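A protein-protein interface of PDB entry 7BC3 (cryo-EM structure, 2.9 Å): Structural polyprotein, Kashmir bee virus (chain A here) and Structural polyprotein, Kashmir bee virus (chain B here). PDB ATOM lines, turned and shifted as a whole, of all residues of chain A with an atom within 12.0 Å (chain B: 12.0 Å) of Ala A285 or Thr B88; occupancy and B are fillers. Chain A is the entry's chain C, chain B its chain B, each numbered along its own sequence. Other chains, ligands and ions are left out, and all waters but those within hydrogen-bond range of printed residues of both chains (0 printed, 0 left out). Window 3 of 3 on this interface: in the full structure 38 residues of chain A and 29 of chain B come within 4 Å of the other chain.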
ATOM      1  N   ARG A 103      -8.112  39.600  26.667  1.00  0.00           N
ATOM      2  CA  ARG A 103      -8.891  38.765  27.570  1.00  0.00           C
ATOM      3  C   ARG A 103      -8.745  39.330  28.977  1.00  0.00           C
ATOM      4  O   ARG A 103      -7.660  39.280  29.564  1.00  0.00           O
ATOM      5  CB  ARG A 103      -8.423  37.315  27.509  1.00  0.00           C
ATOM      6  CG  ARG A 103      -9.118  36.418  28.503  1.00  0.00           C
ATOM      7  CD  ARG A 103      -8.813  34.964  28.242  1.00  0.00           C
ATOM      8  NE  ARG A 103      -9.492  34.093  29.194  1.00  0.00           N
ATOM      9  CZ  ARG A 103      -8.996  33.741  30.374  1.00  0.00           C
ATOM     10  NH1 ARG A 103      -9.695  32.946  31.169  1.00  0.00           N
ATOM     11  NH2 ARG A 103      -7.807  34.179  30.766  1.00  0.00           N
ATOM     12  N   ALA A 104      -9.834  39.870  29.515  1.00  0.00           N
ATOM     13  CA  ALA A 104      -9.841  40.494  30.829  1.00  0.00           C
ATOM     14  C   ALA A 104     -10.592  39.593  31.797  1.00  0.00           C
ATOM     15  O   ALA A 104     -11.781  39.321  31.603  1.00  0.00           O
ATOM     16  CB  ALA A 104     -10.483  41.879  30.773  1.00  0.00           C
ATOM     17  N   VAL A 105      -9.896  39.130  32.832  1.00  0.00           N
ATOM     18  CA  VAL A 105     -10.475  38.263  33.847  1.00  0.00           C
ATOM     19  C   VAL A 105     -10.051  38.764  35.218  1.00  0.00           C
ATOM     20  O   VAL A 105      -8.981  39.359  35.382  1.00  0.00           O
ATOM     21  CB  VAL A 105     -10.056  36.790  33.654  1.00  0.00           C
ATOM     22  CG1 VAL A 105      -8.555  36.635  33.830  1.00  0.00           C
ATOM     23  CG2 VAL A 105     -10.811  35.891  34.620  1.00  0.00           C
ATOM     24  N   TYR A 281      -0.522  30.890  23.562  1.00  0.00           N
ATOM     25  CA  TYR A 281      -1.745  30.999  24.344  1.00  0.00           C
ATOM     26  C   TYR A 281      -2.451  29.652  24.360  1.00  0.00           C
ATOM     27  O   TYR A 281      -2.855  29.142  23.309  1.00  0.00           O
ATOM     28  CB  TYR A 281      -2.656  32.078  23.766  1.00  0.00           C
ATOM     29  CG  TYR A 281      -3.910  32.303  24.572  1.00  0.00           C
ATOM     30  CD1 TYR A 281      -3.860  32.928  25.807  1.00  0.00           C
ATOM     31  CD2 TYR A 281      -5.145  31.888  24.098  1.00  0.00           C
ATOM     32  CE1 TYR A 281      -5.003  33.135  26.547  1.00  0.00           C
ATOM     33  CE2 TYR A 281      -6.291  32.091  24.831  1.00  0.00           C
ATOM     34  CZ  TYR A 281      -6.215  32.713  26.053  1.00  0.00           C
ATOM     35  OH  TYR A 281      -7.361  32.915  26.783  1.00  0.00           O
ATOM     36  N   ASN A 282      -2.592  29.074  25.550  1.00  0.00           N
ATOM     37  CA  ASN A 282      -3.331  27.836  25.728  1.00  0.00           C
ATOM     38  C   ASN A 282      -4.711  28.189  26.265  1.00  0.00           C
ATOM     39  O   ASN A 282      -4.845  28.479  27.464  1.00  0.00           O
ATOM     40  CB  ASN A 282      -2.597  26.898  26.686  1.00  0.00           C
ATOM     41  CG  ASN A 282      -1.201  26.553  26.206  1.00  0.00           C
ATOM     42  OD1 ASN A 282      -0.938  26.520  25.005  1.00  0.00           O
ATOM     43  ND2 ASN A 282      -0.298  26.298  27.143  1.00  0.00           N
ATOM     44  N   PRO A 283      -5.755  28.196  25.441  1.00  0.00           N
ATOM     45  CA  PRO A 283      -7.066  28.641  25.914  1.00  0.00           C
ATOM     46  C   PRO A 283      -7.529  27.810  27.096  1.00  0.00           C
ATOM     47  O   PRO A 283      -7.608  26.577  27.003  1.00  0.00           O
ATOM     48  CB  PRO A 283      -7.972  28.432  24.693  1.00  0.00           C
ATOM     49  CG  PRO A 283      -7.058  28.442  23.540  1.00  0.00           C
ATOM     50  CD  PRO A 283      -5.800  27.807  24.022  1.00  0.00           C
ATOM     51  N   PRO A 284      -7.840  28.441  28.224  1.00  0.00           N
ATOM     52  CA  PRO A 284      -8.278  27.677  29.395  1.00  0.00           C
ATOM     53  C   PRO A 284      -9.606  26.981  29.144  1.00  0.00           C
ATOM     54  O   PRO A 284     -10.277  27.179  28.131  1.00  0.00           O
ATOM     55  CB  PRO A 284      -8.402  28.735  30.490  1.00  0.00           C
ATOM     56  CG  PRO A 284      -8.504  30.026  29.781  1.00  0.00           C
ATOM     57  CD  PRO A 284      -7.720  29.877  28.528  1.00  0.00           C
ATOM     58  N   ALA A 285      -9.982  26.143  30.112  1.00  0.00           N
ATOM     59  CA  ALA A 285     -11.217  25.379  29.989  1.00  0.00           C
ATOM     60  C   ALA A 285     -12.439  26.288  30.013  1.00  0.00           C
ATOM     61  O   ALA A 285     -13.381  26.089  29.239  1.00  0.00           O
ATOM     62  CB  ALA A 285     -11.299  24.344  31.107  1.00  0.00           C
ATOM     63  N   VAL A 286     -12.441  27.289  30.893  1.00  0.00           N
ATOM     64  CA  VAL A 286     -13.551  28.220  31.027  1.00  0.00           C
ATOM     65  C   VAL A 286     -12.999  29.640  31.027  1.00  0.00           C
ATOM     66  O   VAL A 286     -11.789  29.864  30.998  1.00  0.00           O
ATOM     67  CB  VAL A 286     -14.385  27.960  32.299  1.00  0.00           C
ATOM     68  CG1 VAL A 286     -15.147  26.650  32.175  1.00  0.00           C
ATOM     69  CG2 VAL A 286     -13.496  27.957  33.535  1.00  0.00           C
ATOM     70  N   ALA A 287     -13.915  30.605  31.059  1.00  0.00           N
ATOM     71  CA  ALA A 287     -13.557  32.016  31.017  1.00  0.00           C
ATOM     72  C   ALA A 287     -13.089  32.556  32.362  1.00  0.00           C
ATOM     73  O   ALA A 287     -12.693  33.724  32.435  1.00  0.00           O
ATOM     74  CB  ALA A 287     -14.749  32.839  30.524  1.00  0.00           C
ATOM     75  N   ARG A 288     -13.122  31.747  33.420  1.00  0.00           N
ATOM     76  CA  ARG A 288     -12.706  32.194  34.742  1.00  0.00           C
ATOM     77  C   ARG A 288     -11.224  31.976  35.008  1.00  0.00           C
ATOM     78  O   ARG A 288     -10.693  32.543  35.970  1.00  0.00           O
ATOM     79  CB  ARG A 288     -13.505  31.465  35.829  1.00  0.00           C
ATOM     80  CG  ARG A 288     -15.012  31.441  35.617  1.00  0.00           C
ATOM     81  CD  ARG A 288     -15.679  32.686  36.181  1.00  0.00           C
ATOM     82  NE  ARG A 288     -15.181  33.907  35.554  1.00  0.00           N
ATOM     83  CZ  ARG A 288     -15.479  34.287  34.316  1.00  0.00           C
ATOM     84  NH1 ARG A 288     -16.279  33.544  33.562  1.00  0.00           N
ATOM     85  NH2 ARG A 288     -14.977  35.414  33.830  1.00  0.00           N
ATOM     86  N   ASP A 289     -10.548  31.179  34.188  1.00  0.00           N
ATOM     87  CA  ASP A 289      -9.179  30.776  34.473  1.00  0.00           C
ATOM     88  C   ASP A 289      -8.202  31.838  33.973  1.00  0.00           C
ATOM     89  O   ASP A 289      -8.580  32.822  33.332  1.00  0.00           O
ATOM     90  CB  ASP A 289      -8.895  29.417  33.848  1.00  0.00           C
ATOM     91  CG  ASP A 289      -9.962  28.391  34.174  1.00  0.00           C
ATOM     92  OD1 ASP A 289     -10.572  28.490  35.259  1.00  0.00           O
ATOM     93  OD2 ASP A 289     -10.193  27.486  33.346  1.00  0.00           O
ATOM     94  N   LEU A 290      -6.923  31.639  34.275  1.00  0.00           N
ATOM     95  CA  LEU A 290      -5.891  32.620  33.965  1.00  0.00           C
ATOM     96  C   LEU A 290      -4.676  31.942  33.342  1.00  0.00           C
ATOM     97  O   LEU A 290      -4.518  31.928  32.120  1.00  0.00           O
ATOM     98  CB  LEU A 290      -5.477  33.379  35.230  1.00  0.00           C
ATOM     99  CG  LEU A 290      -6.385  34.519  35.706  1.00  0.00           C
ATOM    100  CD1 LEU A 290      -7.653  34.015  36.386  1.00  0.00           C
ATOM    101  CD2 LEU A 290      -5.628  35.433  36.649  1.00  0.00           C
ATOM    102  N   ASP B  75     -24.418  25.940  14.187  1.00  0.00           N
ATOM    103  CA  ASP B  75     -23.001  25.667  13.986  1.00  0.00           C
ATOM    104  C   ASP B  75     -22.686  25.427  12.517  1.00  0.00           C
ATOM    105  O   ASP B  75     -21.554  25.660  12.079  1.00  0.00           O
ATOM    106  CB  ASP B  75     -22.574  24.463  14.824  1.00  0.00           C
ATOM    107  CG  ASP B  75     -22.727  24.705  16.314  1.00  0.00           C
ATOM    108  OD1 ASP B  75     -22.657  25.876  16.738  1.00  0.00           O
ATOM    109  OD2 ASP B  75     -22.918  23.722  17.059  1.00  0.00           O
ATOM    110  N   THR B  78     -22.643  29.129  11.438  1.00  0.00           N
ATOM    111  CA  THR B  78     -21.866  30.053  12.248  1.00  0.00           C
ATOM    112  C   THR B  78     -20.469  30.190  11.662  1.00  0.00           C
ATOM    113  O   THR B  78     -19.763  29.195  11.472  1.00  0.00           O
ATOM    114  CB  THR B  78     -21.787  29.571  13.696  1.00  0.00           C
ATOM    115  OG1 THR B  78     -23.107  29.300  14.184  1.00  0.00           O
ATOM    116  CG2 THR B  78     -21.135  30.625  14.570  1.00  0.00           C
ATOM    117  N   SER B  81     -14.507  32.044  13.694  1.00  0.00           N
ATOM    118  CA  SER B  81     -14.261  33.174  14.576  1.00  0.00           C
ATOM    119  C   SER B  81     -12.809  33.626  14.502  1.00  0.00           C
ATOM    120  O   SER B  81     -11.900  32.832  14.244  1.00  0.00           O
ATOM    121  CB  SER B  81     -14.610  32.819  16.020  1.00  0.00           C
ATOM    122  OG  SER B  81     -14.652  33.979  16.830  1.00  0.00           O
ATOM    123  N   TYR B  83     -10.910  34.942  17.013  1.00  0.00           N
ATOM    124  CA  TYR B  83     -10.147  34.556  18.187  1.00  0.00           C
ATOM    125  C   TYR B  83     -10.851  33.429  18.929  1.00  0.00           C
ATOM    126  O   TYR B  83     -12.056  33.212  18.784  1.00  0.00           O
ATOM    127  CB  TYR B  83      -9.948  35.745  19.134  1.00  0.00           C
ATOM    128  CG  TYR B  83      -9.208  36.899  18.510  1.00  0.00           C
ATOM    129  CD1 TYR B  83      -7.838  36.846  18.324  1.00  0.00           C
ATOM    130  CD2 TYR B  83      -9.880  38.040  18.104  1.00  0.00           C
ATOM    131  CE1 TYR B  83      -7.157  37.894  17.755  1.00  0.00           C
ATOM    132  CE2 TYR B  83      -9.207  39.095  17.531  1.00  0.00           C
ATOM    133  CZ  TYR B  83      -7.845  39.017  17.358  1.00  0.00           C
ATOM    134  OH  TYR B  83      -7.167  40.066  16.786  1.00  0.00           O
ATOM    135  N   VAL B  84     -10.067  32.711  19.730  1.00  0.00           N
ATOM    136  CA  VAL B  84     -10.592  31.676  20.611  1.00  0.00           C
ATOM    137  C   VAL B  84      -9.926  31.832  21.969  1.00  0.00           C
ATOM    138  O   VAL B  84      -8.799  31.370  22.179  1.00  0.00           O
ATOM    139  CB  VAL B  84     -10.363  30.272  20.029  1.00  0.00           C
ATOM    140  CG1 VAL B  84     -10.829  29.212  21.009  1.00  0.00           C
ATOM    141  CG2 VAL B  84     -11.082  30.139  18.704  1.00  0.00           C
ATOM    142  N   LEU B  85     -10.621  32.485  22.894  1.00  0.00           N
ATOM    143  CA  LEU B  85     -10.063  32.796  24.202  1.00  0.00           C
ATOM    144  C   LEU B  85     -10.330  31.706  25.225  1.00  0.00           C
ATOM    145  O   LEU B  85      -9.560  31.561  26.181  1.00  0.00           O
ATOM    146  CB  LEU B  85     -10.643  34.117  24.708  1.00  0.00           C
ATOM    147  CG  LEU B  85     -10.617  35.276  23.711  1.00  0.00           C
ATOM    148  CD1 LEU B  85     -11.005  36.569  24.393  1.00  0.00           C
ATOM    149  CD2 LEU B  85      -9.253  35.403  23.065  1.00  0.00           C
ATOM    150  N   ASP B  86     -11.398  30.938  25.043  1.00  0.00           N
ATOM    151  CA  ASP B  86     -11.790  29.900  25.978  1.00  0.00           C
ATOM    152  C   ASP B  86     -12.211  28.661  25.208  1.00  0.00           C
ATOM    153  O   ASP B  86     -12.664  28.744  24.064  1.00  0.00           O
ATOM    154  CB  ASP B  86     -12.935  30.373  26.872  1.00  0.00           C
ATOM    155  CG  ASP B  86     -12.540  31.538  27.752  1.00  0.00           C
ATOM    156  OD1 ASP B  86     -11.374  31.581  28.198  1.00  0.00           O
ATOM    157  OD2 ASP B  86     -13.391  32.420  27.985  1.00  0.00           O
ATOM    158  N   ARG B  87     -12.054  27.503  25.849  1.00  0.00           N
ATOM    159  CA  ARG B  87     -12.512  26.258  25.254  1.00  0.00           C
ATOM    160  C   ARG B  87     -14.026  26.121  25.293  1.00  0.00           C
ATOM    161  O   ARG B  87     -14.563  25.187  24.690  1.00  0.00           O
ATOM    162  CB  ARG B  87     -11.860  25.073  25.962  1.00  0.00           C
ATOM    163  CG  ARG B  87     -10.436  24.815  25.512  1.00  0.00           C
ATOM    164  CD  ARG B  87      -9.738  23.817  26.404  1.00  0.00           C
ATOM    165  NE  ARG B  87      -8.423  24.295  26.815  1.00  0.00           N
ATOM    166  CZ  ARG B  87      -7.740  23.819  27.850  1.00  0.00           C
ATOM    167  NH1 ARG B  87      -8.244  22.842  28.592  1.00  0.00           N
ATOM    168  NH2 ARG B  87      -6.550  24.321  28.145  1.00  0.00           N
ATOM    169  N   THR B  88     -14.719  27.018  25.994  1.00  0.00           N
ATOM    170  CA  THR B  88     -16.171  27.086  25.939  1.00  0.00           C
ATOM    171  C   THR B  88     -16.671  27.834  24.712  1.00  0.00           C
ATOM    172  O   THR B  88     -17.877  27.820  24.445  1.00  0.00           O
ATOM    173  CB  THR B  88     -16.713  27.764  27.197  1.00  0.00           C
ATOM    174  OG1 THR B  88     -15.939  28.937  27.477  1.00  0.00           O
ATOM    175  CG2 THR B  88     -16.640  26.822  28.383  1.00  0.00           C
ATOM    176  N   ASN B  89     -15.775  28.479  23.967  1.00  0.00           N
ATOM    177  CA  ASN B  89     -16.113  29.202  22.744  1.00  0.00           C
ATOM    178  C   ASN B  89     -15.232  28.711  21.600  1.00  0.00           C
ATOM    179  O   ASN B  89     -14.523  29.500  20.963  1.00  0.00           O
ATOM    180  CB  ASN B  89     -15.948  30.705  22.948  1.00  0.00           C
ATOM    181  CG  ASN B  89     -16.945  31.270  23.935  1.00  0.00           C
ATOM    182  OD1 ASN B  89     -18.120  30.906  23.925  1.00  0.00           O
ATOM    183  ND2 ASN B  89     -16.478  32.161  24.800  1.00  0.00           N
ATOM    184  N   PRO B  90     -15.249  27.412  21.314  1.00  0.00           N
ATOM    185  CA  PRO B  90     -14.387  26.879  20.257  1.00  0.00           C
ATOM    186  C   PRO B  90     -14.909  27.226  18.874  1.00  0.00           C
ATOM    187  O   PRO B  90     -16.011  27.749  18.695  1.00  0.00           O
ATOM    188  CB  PRO B  90     -14.426  25.372  20.498  1.00  0.00           C
ATOM    189  CG  PRO B  90     -15.727  25.130  21.150  1.00  0.00           C
ATOM    190  CD  PRO B  90     -16.031  26.350  21.970  1.00  0.00           C
ATOM    191  N   GLN B  91     -14.084  26.919  17.880  1.00  0.00           N
ATOM    192  CA  GLN B  91     -14.508  27.056  16.497  1.00  0.00           C
ATOM    193  C   GLN B  91     -15.584  26.028  16.184  1.00  0.00           C
ATOM    194  O   GLN B  91     -15.424  24.837  16.466  1.00  0.00           O
ATOM    195  CB  GLN B  91     -13.320  26.880  15.556  1.00  0.00           C
ATOM    196  CG  GLN B  91     -12.274  27.968  15.669  1.00  0.00           C
ATOM    197  CD  GLN B  91     -12.768  29.309  15.174  1.00  0.00           C
ATOM    198  OE1 GLN B  91     -13.942  29.469  14.844  1.00  0.00           O
ATOM    199  NE2 GLN B  91     -11.872  30.282  15.121  1.00  0.00           N
ATOM    200  N   LYS B  92     -16.684  26.492  15.606  1.00  0.00           N
ATOM    201  CA  LYS B  92     -17.797  25.625  15.268  1.00  0.00           C
ATOM    202  C   LYS B  92     -17.632  25.098  13.851  1.00  0.00           C
ATOM    203  O   LYS B  92     -17.177  25.814  12.956  1.00  0.00           O
ATOM    204  CB  LYS B  92     -19.118  26.376  15.404  1.00  0.00           C
ATOM    205  CG  LYS B  92     -19.525  26.596  16.844  1.00  0.00           C
ATOM    206  CD  LYS B  92     -20.325  27.867  17.012  1.00  0.00           C
ATOM    207  CE  LYS B  92     -20.467  28.224  18.475  1.00  0.00           C
ATOM    208  NZ  LYS B  92     -21.099  29.556  18.654  1.00  0.00           N
ATOM    209  N   TYR B  93     -18.003  23.836  13.657  1.00  0.00           N
ATOM    210  CA  TYR B  93     -17.852  23.168  12.377  1.00  0.00           C
ATOM    211  C   TYR B  93     -19.204  22.668  11.899  1.00  0.00           C
ATOM    212  O   TYR B  93     -20.141  22.491  12.680  1.00  0.00           O
ATOM    213  CB  TYR B  93     -16.863  21.997  12.465  1.00  0.00           C
ATOM    214  CG  TYR B  93     -17.155  21.021  13.580  1.00  0.00           C
ATOM    215  CD1 TYR B  93     -16.503  21.114  14.799  1.00  0.00           C
ATOM    216  CD2 TYR B  93     -18.077  20.000  13.409  1.00  0.00           C
ATOM    217  CE1 TYR B  93     -16.764  20.224  15.818  1.00  0.00           C
ATOM    218  CE2 TYR B  93     -18.346  19.105  14.421  1.00  0.00           C
ATOM    219  CZ  TYR B  93     -17.686  19.220  15.625  1.00  0.00           C
ATOM    220  OH  TYR B  93     -17.949  18.330  16.639  1.00  0.00           O
ATOM    221  N   ALA B 151      -2.858  17.691  22.453  1.00  0.00           N
ATOM    222  CA  ALA B 151      -3.284  18.653  23.453  1.00  0.00           C
ATOM    223  C   ALA B 151      -4.224  19.685  22.828  1.00  0.00           C
ATOM    224  O   ALA B 151      -4.134  19.974  21.631  1.00  0.00           O
ATOM    225  CB  ALA B 151      -2.076  19.353  24.069  1.00  0.00           C
ATOM    226  N   PRO B 152      -5.136  20.260  23.617  1.00  0.00           N
ATOM    227  CA  PRO B 152      -6.099  21.209  23.033  1.00  0.00           C
ATOM    228  C   PRO B 152      -5.445  22.431  22.417  1.00  0.00           C
ATOM    229  O   PRO B 152      -5.886  22.897  21.360  1.00  0.00           O
ATOM    230  CB  PRO B 152      -6.989  21.579  24.228  1.00  0.00           C
ATOM    231  CG  PRO B 152      -6.156  21.298  25.424  1.00  0.00           C
ATOM    232  CD  PRO B 152      -5.337  20.102  25.067  1.00  0.00           C
ATOM    233  N   GLU B 153      -4.403  22.969  23.050  1.00  0.00           N
ATOM    234  CA  GLU B 153      -3.715  24.129  22.500  1.00  0.00           C
ATOM    235  C   GLU B 153      -3.104  23.855  21.134  1.00  0.00           C
ATOM    236  O   GLU B 153      -2.666  24.802  20.470  1.00  0.00           O
ATOM    237  CB  GLU B 153      -2.629  24.605  23.468  1.00  0.00           C
ATOM    238  CG  GLU B 153      -1.576  23.558  23.809  1.00  0.00           C
ATOM    239  CD  GLU B 153      -1.917  22.757  25.052  1.00  0.00           C
ATOM    240  OE1 GLU B 153      -3.096  22.767  25.464  1.00  0.00           O
ATOM    241  OE2 GLU B 153      -1.005  22.120  25.616  1.00  0.00           O
ATOM    242  N   ARG B 155      -4.893  21.828  18.841  1.00  0.00           N
ATOM    243  CA  ARG B 155      -5.979  21.377  17.991  1.00  0.00           C
ATOM    244  C   ARG B 155      -6.357  22.456  16.985  1.00  0.00           C
ATOM    245  O   ARG B 155      -6.151  23.653  17.205  1.00  0.00           O
ATOM    246  CB  ARG B 155      -7.197  21.005  18.833  1.00  0.00           C
ATOM    247  CG  ARG B 155      -6.997  19.773  19.691  1.00  0.00           C
ATOM    248  CD  ARG B 155      -8.193  19.511  20.583  1.00  0.00           C
ATOM    249  NE  ARG B 155      -9.337  18.997  19.838  1.00  0.00           N
ATOM    250  CZ  ARG B 155     -10.455  18.552  20.403  1.00  0.00           C
ATOM    251  NH1 ARG B 155     -10.584  18.555  21.722  1.00  0.00           N
ATOM    252  NH2 ARG B 155     -11.444  18.101  19.646  1.00  0.00           N
ATOM    253  N   ILE B 157      -9.421  22.998  16.335  1.00  0.00           N
ATOM    254  CA  ILE B 157     -10.275  23.694  17.279  1.00  0.00           C
ATOM    255  C   ILE B 157      -9.404  24.314  18.364  1.00  0.00           C
ATOM    256  O   ILE B 157      -8.290  23.858  18.645  1.00  0.00           O
ATOM    257  CB  ILE B 157     -11.322  22.743  17.882  1.00  0.00           C
ATOM    258  CG1 ILE B 157     -11.969  21.883  16.797  1.00  0.00           C
ATOM    259  CG2 ILE B 157     -12.391  23.525  18.615  1.00  0.00           C
ATOM    260  CD1 ILE B 157     -12.473  22.664  15.621  1.00  0.00           C
ATOM    261  N   TYR B 158      -9.913  25.381  18.972  1.00  0.00           N
ATOM    262  CA  TYR B 158      -9.229  26.122  20.026  1.00  0.00           C
ATOM    263  C   TYR B 158      -8.108  27.004  19.492  1.00  0.00           C
ATOM    264  O   TYR B 158      -7.297  27.502  20.281  1.00  0.00           O
ATOM    265  CB  TYR B 158      -8.664  25.190  21.105  1.00  0.00           C
ATOM    266  CG  TYR B 158      -9.675  24.224  21.674  1.00  0.00           C
ATOM    267  CD1 TYR B 158     -10.991  24.606  21.877  1.00  0.00           C
ATOM    268  CD2 TYR B 158      -9.313  22.929  22.011  1.00  0.00           C
ATOM    269  CE1 TYR B 158     -11.918  23.728  22.398  1.00  0.00           C
ATOM    270  CE2 TYR B 158     -10.234  22.043  22.533  1.00  0.00           C
ATOM    271  CZ  TYR B 158     -11.535  22.449  22.725  1.00  0.00           C
ATOM    272  OH  TYR B 158     -12.464  21.579  23.244  1.00  0.00           O
ATOM    273  N   THR B 159      -8.034  27.207  18.177  1.00  0.00           N
ATOM    274  CA  THR B 159      -7.129  28.200  17.613  1.00  0.00           C
ATOM    275  C   THR B 159      -7.914  29.171  16.743  1.00  0.00           C
ATOM    276  O   THR B 159      -9.148  29.142  16.730  1.00  0.00           O
ATOM    277  CB  THR B 159      -6.002  27.546  16.808  1.00  0.00           C
ATOM    278  OG1 THR B 159      -5.119  28.560  16.314  1.00  0.00           O
ATOM    279  CG2 THR B 159      -6.542  26.755  15.639  1.00  0.00           C
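Of chain A, only Ala A285 comes within 4 Å of Thr B88. Pro A283 touches four residues of chain B. Pro A284 touches just these residues of chain B: Leu B85 (3.4 Å), Asp B86 (3.6 Å) and Arg B87 (2.9 Å). Ala A287 touches one residue of chain B. No residue of chain B comes within 4 Å of Asp A289. Asp B86 touches four residues of chain A. Arg B87 touches just these residues of chain A: Pro A283, Pro A284 and Ala A285. No residue of chain A comes within 4 Å of Asn B89. No residue of chain A comes within 4 Å of Pro B90. Printed residues of chain A within 4 Å of Leu B85: Arg A103, Tyr A281, Pro A283 and Pro A284. Of the printed residues of chain A, Tyr B158 touches Pro A283 (3.4 Å). Printed residues of chain B within 4 Å of Asn A282: Glu B153. Of the printed residues of chain A, Glu B153 touches Asn A282. Printed residues of chain B within 4 Å of Tyr A281: Val B84 and Leu B85.
The side-chain carboxylate (OD1) of Asp B86 is in salt-bridge range of the guanidinium group (NE) of Arg A103 (3.3 Å). O of Leu B85 is in hydrogen-bond range of OH of Tyr A281 (2.7 Å). O of Pro A283 lies within hydrogen-bond range of NE of Arg B87, at 2.4 Å. The side-chain carboxylate of Asp B86 lies close to the backbone carbonyl oxygen of Val A286 (3.3 Å). O of Pro A284 is in hydrogen-bond range of N of Arg B87, 2.9 Å away.
Among the printed residues, pairs that only touch across the chains: Ala A287 with Asp B86, Asn A282 with Glu B153, Pro A283 with Tyr B158, Pro A284 with Leu B85, Ala A285 with Thr B88, Pro A284 with Asp B86, Pro A283 with Val B84, Tyr A281 with Val B84, Ala A285 with Arg B87, Pro A283 with Leu B85 and Arg A103 with Leu B85.
Hydrophobic or aromatic side chains of chain A within 4 Å of the printed part of chain B: Tyr A281, Pro A283, Pro A284 and Ala A287. Along chain A the printed residues that touch a printed residue of chain B span positions 103 to 287.
The guanidinium group (NH1) of Arg A103 sits at hydrogen-bond distance from the backbone carbonyl oxygen (O) of Ala A287, 3.3 Å away. The guanidinium group (NE) of Arg A103 lies close to the side-chain hydroxyl (OH) of Tyr A281, at 3.4 Å. O of Asp A289 sits at hydrogen-bond distance from NH1 of Arg A103, 2.4 Å away. N of Val A286 lies within hydrogen-bond range of OD2 of Asp A289 (3.3 Å).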
